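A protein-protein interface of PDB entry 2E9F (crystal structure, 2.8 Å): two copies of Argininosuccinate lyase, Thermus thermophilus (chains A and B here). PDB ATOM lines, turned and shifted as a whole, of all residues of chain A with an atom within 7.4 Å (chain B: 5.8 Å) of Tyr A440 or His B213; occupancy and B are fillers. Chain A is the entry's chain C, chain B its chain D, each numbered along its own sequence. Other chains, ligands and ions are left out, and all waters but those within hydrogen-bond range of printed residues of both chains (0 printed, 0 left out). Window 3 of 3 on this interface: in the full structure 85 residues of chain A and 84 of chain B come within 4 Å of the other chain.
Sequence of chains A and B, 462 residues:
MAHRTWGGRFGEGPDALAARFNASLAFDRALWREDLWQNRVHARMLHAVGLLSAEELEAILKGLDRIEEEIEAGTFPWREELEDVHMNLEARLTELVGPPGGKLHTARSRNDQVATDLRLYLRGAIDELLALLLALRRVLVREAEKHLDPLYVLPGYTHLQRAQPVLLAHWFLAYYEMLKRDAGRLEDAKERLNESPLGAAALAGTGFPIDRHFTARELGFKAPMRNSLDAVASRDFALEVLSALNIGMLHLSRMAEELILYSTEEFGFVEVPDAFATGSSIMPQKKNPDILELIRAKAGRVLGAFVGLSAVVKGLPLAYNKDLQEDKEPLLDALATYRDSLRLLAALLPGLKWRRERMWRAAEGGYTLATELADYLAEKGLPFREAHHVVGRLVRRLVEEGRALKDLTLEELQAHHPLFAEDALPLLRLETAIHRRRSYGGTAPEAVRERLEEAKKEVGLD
No position is printed for both chains. Of the 14 pairs that touch across the chains among the printed residues, none has its exchanged pair printed and touching as well.
Printed residues of chain B within 4 Å of His A170: Ser B228 (3.1 Å). Of the printed residues of chain B, Ser A439 touches Gly B205. Of the printed residues of chain B, Arg A451 touches Arg B226. His B213 touches just one residue of chain A: Tyr A440 (3.4 Å). Printed residues of chain A within 4 Å of Met B225: Tyr A440. Of the printed residues of chain A, Ser B228 touches His A170 and Gly A441.
Printed residues of chain A that touch a printed residue of chain B: His A170, Arg A437, Ser A439, Tyr A440, Gly A441, Gly A442, Thr A443, Arg A451 and Glu A454. Hydrophobic or aromatic side chains of chain A within 4 Å of the printed part of chain B: His A170 and Tyr A440. Among the printed residues, Asp or Glu carboxylates within 4 Å of a Lys or Arg side-chain nitrogen of the other chain: Glu A454 with Arg B226 (3.7 Å).
His A170 touches Ser B228 (CE1 to OG, 3.1 Å). Ser A439 touches Gly B205 (OG to CA, 3.2 Å). Tyr A440 touches His B213. Tyr A440 touches Pro B224 (CE1 to O, 3.8 Å). Met B225 touches Tyr A440. OH of Tyr A440 touches CG of Arg B226, at 3.5 Å. Arg B226 touches Gly A441 (O to CA, 3.3 Å). Gly A442 touches Gly B205 (CA to N, 3.4 Å). Thr A443 touches Gly B205. Arg A451 touches Arg B226.
NH1 of Arg A437 is in hydrogen-bond range of O of Gly B205 (3.0 Å). The backbone carbonyl oxygen (O) of Tyr A440 is in hydrogen-bond range of the guanidinium group (NH1) of Arg B212, 3.0 Å away. O of Gly A441 is in hydrogen-bond range of N of Ser B228, 3.0 Å away. OE2 of Glu A454 is in salt-bridge range of NH1 of Arg B226 (3.7 Å).
The backbone carbonyl oxygen (O) of Gly A441 lies within hydrogen-bond range of a ring nitrogen (NE2) of His A170. A ring nitrogen (NE2) of His A170 sits at hydrogen-bond distance from the backbone carbonyl oxygen of Gly A442 (3.3 Å). The side-chain carboxylate (OE2) of Glu A450 lies within salt-bridge range of the guanidinium group (NH2) of Arg A451, 3.1 Å away. The side-chain carboxylate (OE2) of Glu A454 lies within salt-bridge range of the guanidinium group (NE) of Arg A451 (2.6 Å). O of Arg B212 sits at hydrogen-bond distance from OG1 of Thr B215 (3.1 Å). O of Met B225 sits at hydrogen-bond distance from NH1 of Arg B212, at 2.8 Å.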
ATOM      1  N   HIS A 170       2.103  26.948  -0.107  1.00  0.00           N
ATOM      2  CA  HIS A 170       2.646  25.811  -0.828  1.00  0.00           C
ATOM      3  C   HIS A 170       1.488  25.030  -1.474  1.00  0.00           C
ATOM      4  O   HIS A 170       1.527  24.695  -2.660  1.00  0.00           O
ATOM      5  CB  HIS A 170       3.405  24.903   0.127  1.00  0.00           C
ATOM      6  CG  HIS A 170       4.409  24.037  -0.557  1.00  0.00           C
ATOM      7  ND1 HIS A 170       4.675  22.745  -0.161  1.00  0.00           N
ATOM      8  CD2 HIS A 170       5.216  24.283  -1.615  1.00  0.00           C
ATOM      9  CE1 HIS A 170       5.602  22.230  -0.949  1.00  0.00           C
ATOM     10  NE2 HIS A 170       5.946  23.143  -1.839  1.00  0.00           N
ATOM     11  N   ARG A 437      12.420  22.036   6.013  1.00  0.00           N
ATOM     12  CA  ARG A 437      12.289  21.605   4.618  1.00  0.00           C
ATOM     13  C   ARG A 437      12.609  22.677   3.578  1.00  0.00           C
ATOM     14  O   ARG A 437      11.711  23.067   2.825  1.00  0.00           O
ATOM     15  CB  ARG A 437      10.863  21.116   4.375  1.00  0.00           C
ATOM     16  CG  ARG A 437      10.293  20.280   5.504  1.00  0.00           C
ATOM     17  CD  ARG A 437      10.614  18.833   5.333  1.00  0.00           C
ATOM     18  NE  ARG A 437      10.152  18.057   6.472  1.00  0.00           N
ATOM     19  CZ  ARG A 437      10.230  16.734   6.544  1.00  0.00           C
ATOM     20  NH1 ARG A 437      10.744  16.049   5.530  1.00  0.00           N
ATOM     21  NH2 ARG A 437       9.819  16.096   7.630  1.00  0.00           N
ATOM     22  N   ARG A 438      13.863  23.134   3.491  1.00  0.00           N
ATOM     23  CA  ARG A 438      14.176  24.185   2.522  1.00  0.00           C
ATOM     24  C   ARG A 438      14.813  23.769   1.194  1.00  0.00           C
ATOM     25  O   ARG A 438      15.537  24.546   0.563  1.00  0.00           O
ATOM     26  CB  ARG A 438      14.981  25.330   3.185  1.00  0.00           C
ATOM     27  CG  ARG A 438      16.409  25.045   3.657  1.00  0.00           C
ATOM     28  CD  ARG A 438      17.048  26.302   4.316  1.00  0.00           C
ATOM     29  NE  ARG A 438      17.087  27.478   3.429  1.00  0.00           N
ATOM     30  CZ  ARG A 438      16.322  28.572   3.554  1.00  0.00           C
ATOM     31  NH1 ARG A 438      15.439  28.675   4.546  1.00  0.00           N
ATOM     32  NH2 ARG A 438      16.423  29.560   2.666  1.00  0.00           N
ATOM     33  N   SER A 439      14.508  22.550   0.759  1.00  0.00           N
ATOM     34  CA  SER A 439      15.004  22.038  -0.516  1.00  0.00           C
ATOM     35  C   SER A 439      14.084  22.535  -1.630  1.00  0.00           C
ATOM     36  O   SER A 439      12.926  22.859  -1.375  1.00  0.00           O
ATOM     37  CB  SER A 439      15.020  20.513  -0.493  1.00  0.00           C
ATOM     38  OG  SER A 439      13.804  20.007   0.022  1.00  0.00           O
ATOM     39  N   TYR A 440      14.598  22.597  -2.857  1.00  0.00           N
ATOM     40  CA  TYR A 440      13.811  23.073  -3.994  1.00  0.00           C
ATOM     41  C   TYR A 440      12.436  22.416  -4.001  1.00  0.00           C
ATOM     42  O   TYR A 440      12.326  21.187  -3.994  1.00  0.00           O
ATOM     43  CB  TYR A 440      14.545  22.774  -5.310  1.00  0.00           C
ATOM     44  CG  TYR A 440      13.991  23.492  -6.535  1.00  0.00           C
ATOM     45  CD1 TYR A 440      13.096  22.864  -7.405  1.00  0.00           C
ATOM     46  CD2 TYR A 440      14.348  24.812  -6.808  1.00  0.00           C
ATOM     47  CE1 TYR A 440      12.573  23.541  -8.516  1.00  0.00           C
ATOM     48  CE2 TYR A 440      13.831  25.491  -7.907  1.00  0.00           C
ATOM     49  CZ  TYR A 440      12.945  24.856  -8.758  1.00  0.00           C
ATOM     50  OH  TYR A 440      12.430  25.557  -9.832  1.00  0.00           O
ATOM     51  N   GLY A 441      11.393  23.245  -4.004  1.00  0.00           N
ATOM     52  CA  GLY A 441      10.029  22.737  -4.007  1.00  0.00           C
ATOM     53  C   GLY A 441       9.570  22.291  -2.629  1.00  0.00           C
ATOM     54  O   GLY A 441       8.532  21.637  -2.488  1.00  0.00           O
ATOM     55  N   GLY A 442      10.346  22.644  -1.610  1.00  0.00           N
ATOM     56  CA  GLY A 442      10.009  22.266  -0.252  1.00  0.00           C
ATOM     57  C   GLY A 442       8.931  23.154   0.320  1.00  0.00           C
ATOM     58  O   GLY A 442       8.632  24.204  -0.253  1.00  0.00           O
ATOM     59  N   THR A 443       8.352  22.736   1.444  1.00  0.00           N
ATOM     60  CA  THR A 443       7.290  23.500   2.092  1.00  0.00           C
ATOM     61  C   THR A 443       7.829  24.617   2.981  1.00  0.00           C
ATOM     62  O   THR A 443       7.065  25.454   3.468  1.00  0.00           O
ATOM     63  CB  THR A 443       6.402  22.602   2.969  1.00  0.00           C
ATOM     64  OG1 THR A 443       5.342  23.386   3.527  1.00  0.00           O
ATOM     65  CG2 THR A 443       7.204  21.996   4.101  1.00  0.00           C
ATOM     66  N   ALA A 447      11.623  28.471   0.657  1.00  0.00           N
ATOM     67  CA  ALA A 447      11.475  27.716  -0.576  1.00  0.00           C
ATOM     68  C   ALA A 447      10.242  28.270  -1.292  1.00  0.00           C
ATOM     69  O   ALA A 447      10.331  28.771  -2.416  1.00  0.00           O
ATOM     70  CB  ALA A 447      11.285  26.240  -0.260  1.00  0.00           C
ATOM     71  N   GLU A 450      10.172  31.656  -2.606  1.00  0.00           N
ATOM     72  CA  GLU A 450      10.948  31.675  -3.846  1.00  0.00           C
ATOM     73  C   GLU A 450      10.050  31.339  -5.038  1.00  0.00           C
ATOM     74  O   GLU A 450       9.946  32.107  -6.000  1.00  0.00           O
ATOM     75  CB  GLU A 450      12.087  30.657  -3.759  1.00  0.00           C
ATOM     76  CG  GLU A 450      13.213  30.885  -4.749  1.00  0.00           C
ATOM     77  CD  GLU A 450      14.327  29.868  -4.587  1.00  0.00           C
ATOM     78  OE1 GLU A 450      14.724  29.623  -3.420  1.00  0.00           O
ATOM     79  OE2 GLU A 450      14.802  29.319  -5.614  1.00  0.00           O
ATOM     80  N   ARG A 451       9.408  30.180  -4.964  1.00  0.00           N
ATOM     81  CA  ARG A 451       8.507  29.739  -6.013  1.00  0.00           C
ATOM     82  C   ARG A 451       7.421  30.796  -6.264  1.00  0.00           C
ATOM     83  O   ARG A 451       7.076  31.090  -7.409  1.00  0.00           O
ATOM     84  CB  ARG A 451       7.852  28.422  -5.602  1.00  0.00           C
ATOM     85  CG  ARG A 451       8.811  27.280  -5.367  1.00  0.00           C
ATOM     86  CD  ARG A 451       9.313  26.695  -6.673  1.00  0.00           C
ATOM     87  NE  ARG A 451      10.333  27.521  -7.301  1.00  0.00           N
ATOM     88  CZ  ARG A 451      11.465  27.893  -6.702  1.00  0.00           C
ATOM     89  NH1 ARG A 451      11.710  27.511  -5.454  1.00  0.00           N
ATOM     90  NH2 ARG A 451      12.364  28.626  -7.354  1.00  0.00           N
ATOM     91  N   GLU A 454       8.488  33.375  -8.549  1.00  0.00           N
ATOM     92  CA  GLU A 454       8.687  32.772  -9.867  1.00  0.00           C
ATOM     93  C   GLU A 454       7.337  32.777 -10.586  1.00  0.00           C
ATOM     94  O   GLU A 454       7.238  33.101 -11.775  1.00  0.00           O
ATOM     95  CB  GLU A 454       9.154  31.334  -9.685  1.00  0.00           C
ATOM     96  CG  GLU A 454      10.078  30.799 -10.745  1.00  0.00           C
ATOM     97  CD  GLU A 454      10.531  29.399 -10.403  1.00  0.00           C
ATOM     98  OE1 GLU A 454      11.564  28.931 -10.940  1.00  0.00           O
ATOM     99  OE2 GLU A 454       9.836  28.759  -9.586  1.00  0.00           O
ATOM    100  N   GLY B 199      13.004  13.670  -4.593  1.00  0.00           N
ATOM    101  CA  GLY B 199      13.426  14.664  -3.630  1.00  0.00           C
ATOM    102  C   GLY B 199      12.284  15.472  -3.052  1.00  0.00           C
ATOM    103  O   GLY B 199      12.514  16.422  -2.313  1.00  0.00           O
ATOM    104  N   GLY B 205       9.710  19.149   0.971  1.00  0.00           N
ATOM    105  CA  GLY B 205      11.066  18.637   0.814  1.00  0.00           C
ATOM    106  C   GLY B 205      11.624  17.990   2.070  1.00  0.00           C
ATOM    107  O   GLY B 205      10.949  17.199   2.740  1.00  0.00           O
ATOM    108  N   ASP B 211      20.540  17.478  -3.275  1.00  0.00           N
ATOM    109  CA  ASP B 211      20.682  18.284  -4.489  1.00  0.00           C
ATOM    110  C   ASP B 211      19.766  17.642  -5.522  1.00  0.00           C
ATOM    111  O   ASP B 211      20.178  16.715  -6.232  1.00  0.00           O
ATOM    112  CB  ASP B 211      22.121  18.275  -5.025  1.00  0.00           C
ATOM    113  CG  ASP B 211      22.287  19.164  -6.273  1.00  0.00           C
ATOM    114  OD1 ASP B 211      21.343  19.219  -7.096  1.00  0.00           O
ATOM    115  OD2 ASP B 211      23.354  19.801  -6.447  1.00  0.00           O
ATOM    116  N   ARG B 212      18.526  18.122  -5.612  1.00  0.00           N
ATOM    117  CA  ARG B 212      17.590  17.528  -6.552  1.00  0.00           C
ATOM    118  C   ARG B 212      17.793  17.943  -8.004  1.00  0.00           C
ATOM    119  O   ARG B 212      17.257  17.302  -8.905  1.00  0.00           O
ATOM    120  CB  ARG B 212      16.142  17.760  -6.092  1.00  0.00           C
ATOM    121  CG  ARG B 212      15.709  19.191  -5.882  1.00  0.00           C
ATOM    122  CD  ARG B 212      14.465  19.195  -4.999  1.00  0.00           C
ATOM    123  NE  ARG B 212      13.450  18.260  -5.482  1.00  0.00           N
ATOM    124  CZ  ARG B 212      12.421  18.593  -6.261  1.00  0.00           C
ATOM    125  NH1 ARG B 212      12.243  19.854  -6.657  1.00  0.00           N
ATOM    126  NH2 ARG B 212      11.568  17.658  -6.654  1.00  0.00           N
ATOM    127  N   HIS B 213      18.577  18.997  -8.228  1.00  0.00           N
ATOM    128  CA  HIS B 213      18.884  19.457  -9.583  1.00  0.00           C
ATOM    129  C   HIS B 213      19.929  18.498 -10.146  1.00  0.00           C
ATOM    130  O   HIS B 213      20.061  18.321 -11.358  1.00  0.00           O
ATOM    131  CB  HIS B 213      19.448  20.872  -9.553  1.00  0.00           C
ATOM    132  CG  HIS B 213      18.426  21.923  -9.259  1.00  0.00           C
ATOM    133  ND1 HIS B 213      17.775  22.624 -10.253  1.00  0.00           N
ATOM    134  CD2 HIS B 213      17.930  22.382  -8.085  1.00  0.00           C
ATOM    135  CE1 HIS B 213      16.921  23.470  -9.704  1.00  0.00           C
ATOM    136  NE2 HIS B 213      16.995  23.344  -8.390  1.00  0.00           N
ATOM    137  N   PHE B 214      20.678  17.882  -9.244  1.00  0.00           N
ATOM    138  CA  PHE B 214      21.697  16.923  -9.628  1.00  0.00           C
ATOM    139  C   PHE B 214      20.969  15.681 -10.120  1.00  0.00           C
ATOM    140  O   PHE B 214      21.124  15.277 -11.273  1.00  0.00           O
ATOM    141  CB  PHE B 214      22.572  16.580  -8.418  1.00  0.00           C
ATOM    142  CG  PHE B 214      23.566  15.483  -8.669  1.00  0.00           C
ATOM    143  CD1 PHE B 214      24.690  15.708  -9.453  1.00  0.00           C
ATOM    144  CD2 PHE B 214      23.381  14.222  -8.100  1.00  0.00           C
ATOM    145  CE1 PHE B 214      25.618  14.691  -9.667  1.00  0.00           C
ATOM    146  CE2 PHE B 214      24.294  13.198  -8.303  1.00  0.00           C
ATOM    147  CZ  PHE B 214      25.415  13.428  -9.086  1.00  0.00           C
ATOM    148  N   THR B 215      20.160  15.089  -9.247  1.00  0.00           N
ATOM    149  CA  THR B 215      19.419  13.891  -9.604  1.00  0.00           C
ATOM    150  C   THR B 215      18.498  14.121 -10.805  1.00  0.00           C
ATOM    151  O   THR B 215      18.246  13.205 -11.579  1.00  0.00           O
ATOM    152  CB  THR B 215      18.602  13.358  -8.403  1.00  0.00           C
ATOM    153  OG1 THR B 215      17.835  14.423  -7.827  1.00  0.00           O
ATOM    154  CG2 THR B 215      19.526  12.763  -7.350  1.00  0.00           C
ATOM    155  N   ALA B 216      18.003  15.340 -10.969  1.00  0.00           N
ATOM    156  CA  ALA B 216      17.137  15.646 -12.100  1.00  0.00           C
ATOM    157  C   ALA B 216      17.958  15.607 -13.385  1.00  0.00           C
ATOM    158  O   ALA B 216      17.577  14.969 -14.376  1.00  0.00           O
ATOM    159  CB  ALA B 216      16.522  17.027 -11.932  1.00  0.00           C
ATOM    160  N   ARG B 217      19.088  16.305 -13.356  1.00  0.00           N
ATOM    161  CA  ARG B 217      19.997  16.393 -14.488  1.00  0.00           C
ATOM    162  C   ARG B 217      20.588  15.039 -14.894  1.00  0.00           C
ATOM    163  O   ARG B 217      20.591  14.697 -16.075  1.00  0.00           O
ATOM    164  CB  ARG B 217      21.102  17.408 -14.149  1.00  0.00           C
ATOM    165  CG  ARG B 217      22.358  17.338 -15.000  1.00  0.00           C
ATOM    166  CD  ARG B 217      23.228  18.596 -14.846  1.00  0.00           C
ATOM    167  NE  ARG B 217      23.435  19.037 -13.457  1.00  0.00           N
ATOM    168  CZ  ARG B 217      24.185  18.411 -12.546  1.00  0.00           C
ATOM    169  NH1 ARG B 217      24.827  17.287 -12.847  1.00  0.00           N
ATOM    170  NH2 ARG B 217      24.297  18.924 -11.327  1.00  0.00           N
ATOM    171  N   GLU B 218      21.052  14.254 -13.923  1.00  0.00           N
ATOM    172  CA  GLU B 218      21.656  12.955 -14.227  1.00  0.00           C
ATOM    173  C   GLU B 218      20.680  11.822 -14.560  1.00  0.00           C
ATOM    174  O   GLU B 218      21.099  10.734 -14.953  1.00  0.00           O
ATOM    175  CB  GLU B 218      22.584  12.514 -13.082  1.00  0.00           C
ATOM    176  CG  GLU B 218      23.792  13.442 -12.839  1.00  0.00           C
ATOM    177  CD  GLU B 218      24.655  13.679 -14.088  1.00  0.00           C
ATOM    178  OE1 GLU B 218      25.172  12.696 -14.669  1.00  0.00           O
ATOM    179  OE2 GLU B 218      24.824  14.857 -14.485  1.00  0.00           O
ATOM    180  N   PRO B 224      13.810  19.559 -12.198  1.00  0.00           N
ATOM    181  CA  PRO B 224      13.080  18.905 -11.108  1.00  0.00           C
ATOM    182  C   PRO B 224      11.768  19.658 -10.885  1.00  0.00           C
ATOM    183  O   PRO B 224      11.716  20.877 -11.037  1.00  0.00           O
ATOM    184  CB  PRO B 224      14.039  19.036  -9.928  1.00  0.00           C
ATOM    185  CG  PRO B 224      14.634  20.384 -10.165  1.00  0.00           C
ATOM    186  CD  PRO B 224      14.881  20.423 -11.669  1.00  0.00           C
ATOM    187  N   MET B 225      10.710  18.937 -10.537  1.00  0.00           N
ATOM    188  CA  MET B 225       9.415  19.557 -10.310  1.00  0.00           C
ATOM    189  C   MET B 225       9.443  20.647  -9.237  1.00  0.00           C
ATOM    190  O   MET B 225      10.040  20.476  -8.181  1.00  0.00           O
ATOM    191  CB  MET B 225       8.402  18.469  -9.980  1.00  0.00           C
ATOM    192  CG  MET B 225       8.095  17.604 -11.195  1.00  0.00           C
ATOM    193  SD  MET B 225       6.967  16.240 -10.890  1.00  0.00           S
ATOM    194  CE  MET B 225       5.372  17.096 -10.926  1.00  0.00           C
ATOM    195  N   ARG B 226       8.789  21.768  -9.522  1.00  0.00           N
ATOM    196  CA  ARG B 226       8.759  22.915  -8.618  1.00  0.00           C
ATOM    197  C   ARG B 226       7.918  22.833  -7.329  1.00  0.00           C
ATOM    198  O   ARG B 226       8.018  23.712  -6.467  1.00  0.00           O
ATOM    199  CB  ARG B 226       8.362  24.168  -9.411  1.00  0.00           C
ATOM    200  CG  ARG B 226       9.254  24.417 -10.614  1.00  0.00           C
ATOM    201  CD  ARG B 226       9.127  25.823 -11.184  1.00  0.00           C
ATOM    202  NE  ARG B 226       7.759  26.158 -11.542  1.00  0.00           N
ATOM    203  CZ  ARG B 226       7.409  27.167 -12.339  1.00  0.00           C
ATOM    204  NH1 ARG B 226       8.338  27.947 -12.875  1.00  0.00           N
ATOM    205  NH2 ARG B 226       6.123  27.402 -12.594  1.00  0.00           N
ATOM    206  N   SER B 228       6.755  19.975  -4.285  1.00  0.00           N
ATOM    207  CA  SER B 228       6.750  18.627  -3.709  1.00  0.00           C
ATOM    208  C   SER B 228       5.371  17.981  -3.605  1.00  0.00           C
ATOM    209  O   SER B 228       5.230  16.777  -3.836  1.00  0.00           O
ATOM    210  CB  SER B 228       7.381  18.648  -2.323  1.00  0.00           C
ATOM    211  OG  SER B 228       6.564  19.375  -1.430  1.00  0.00           O
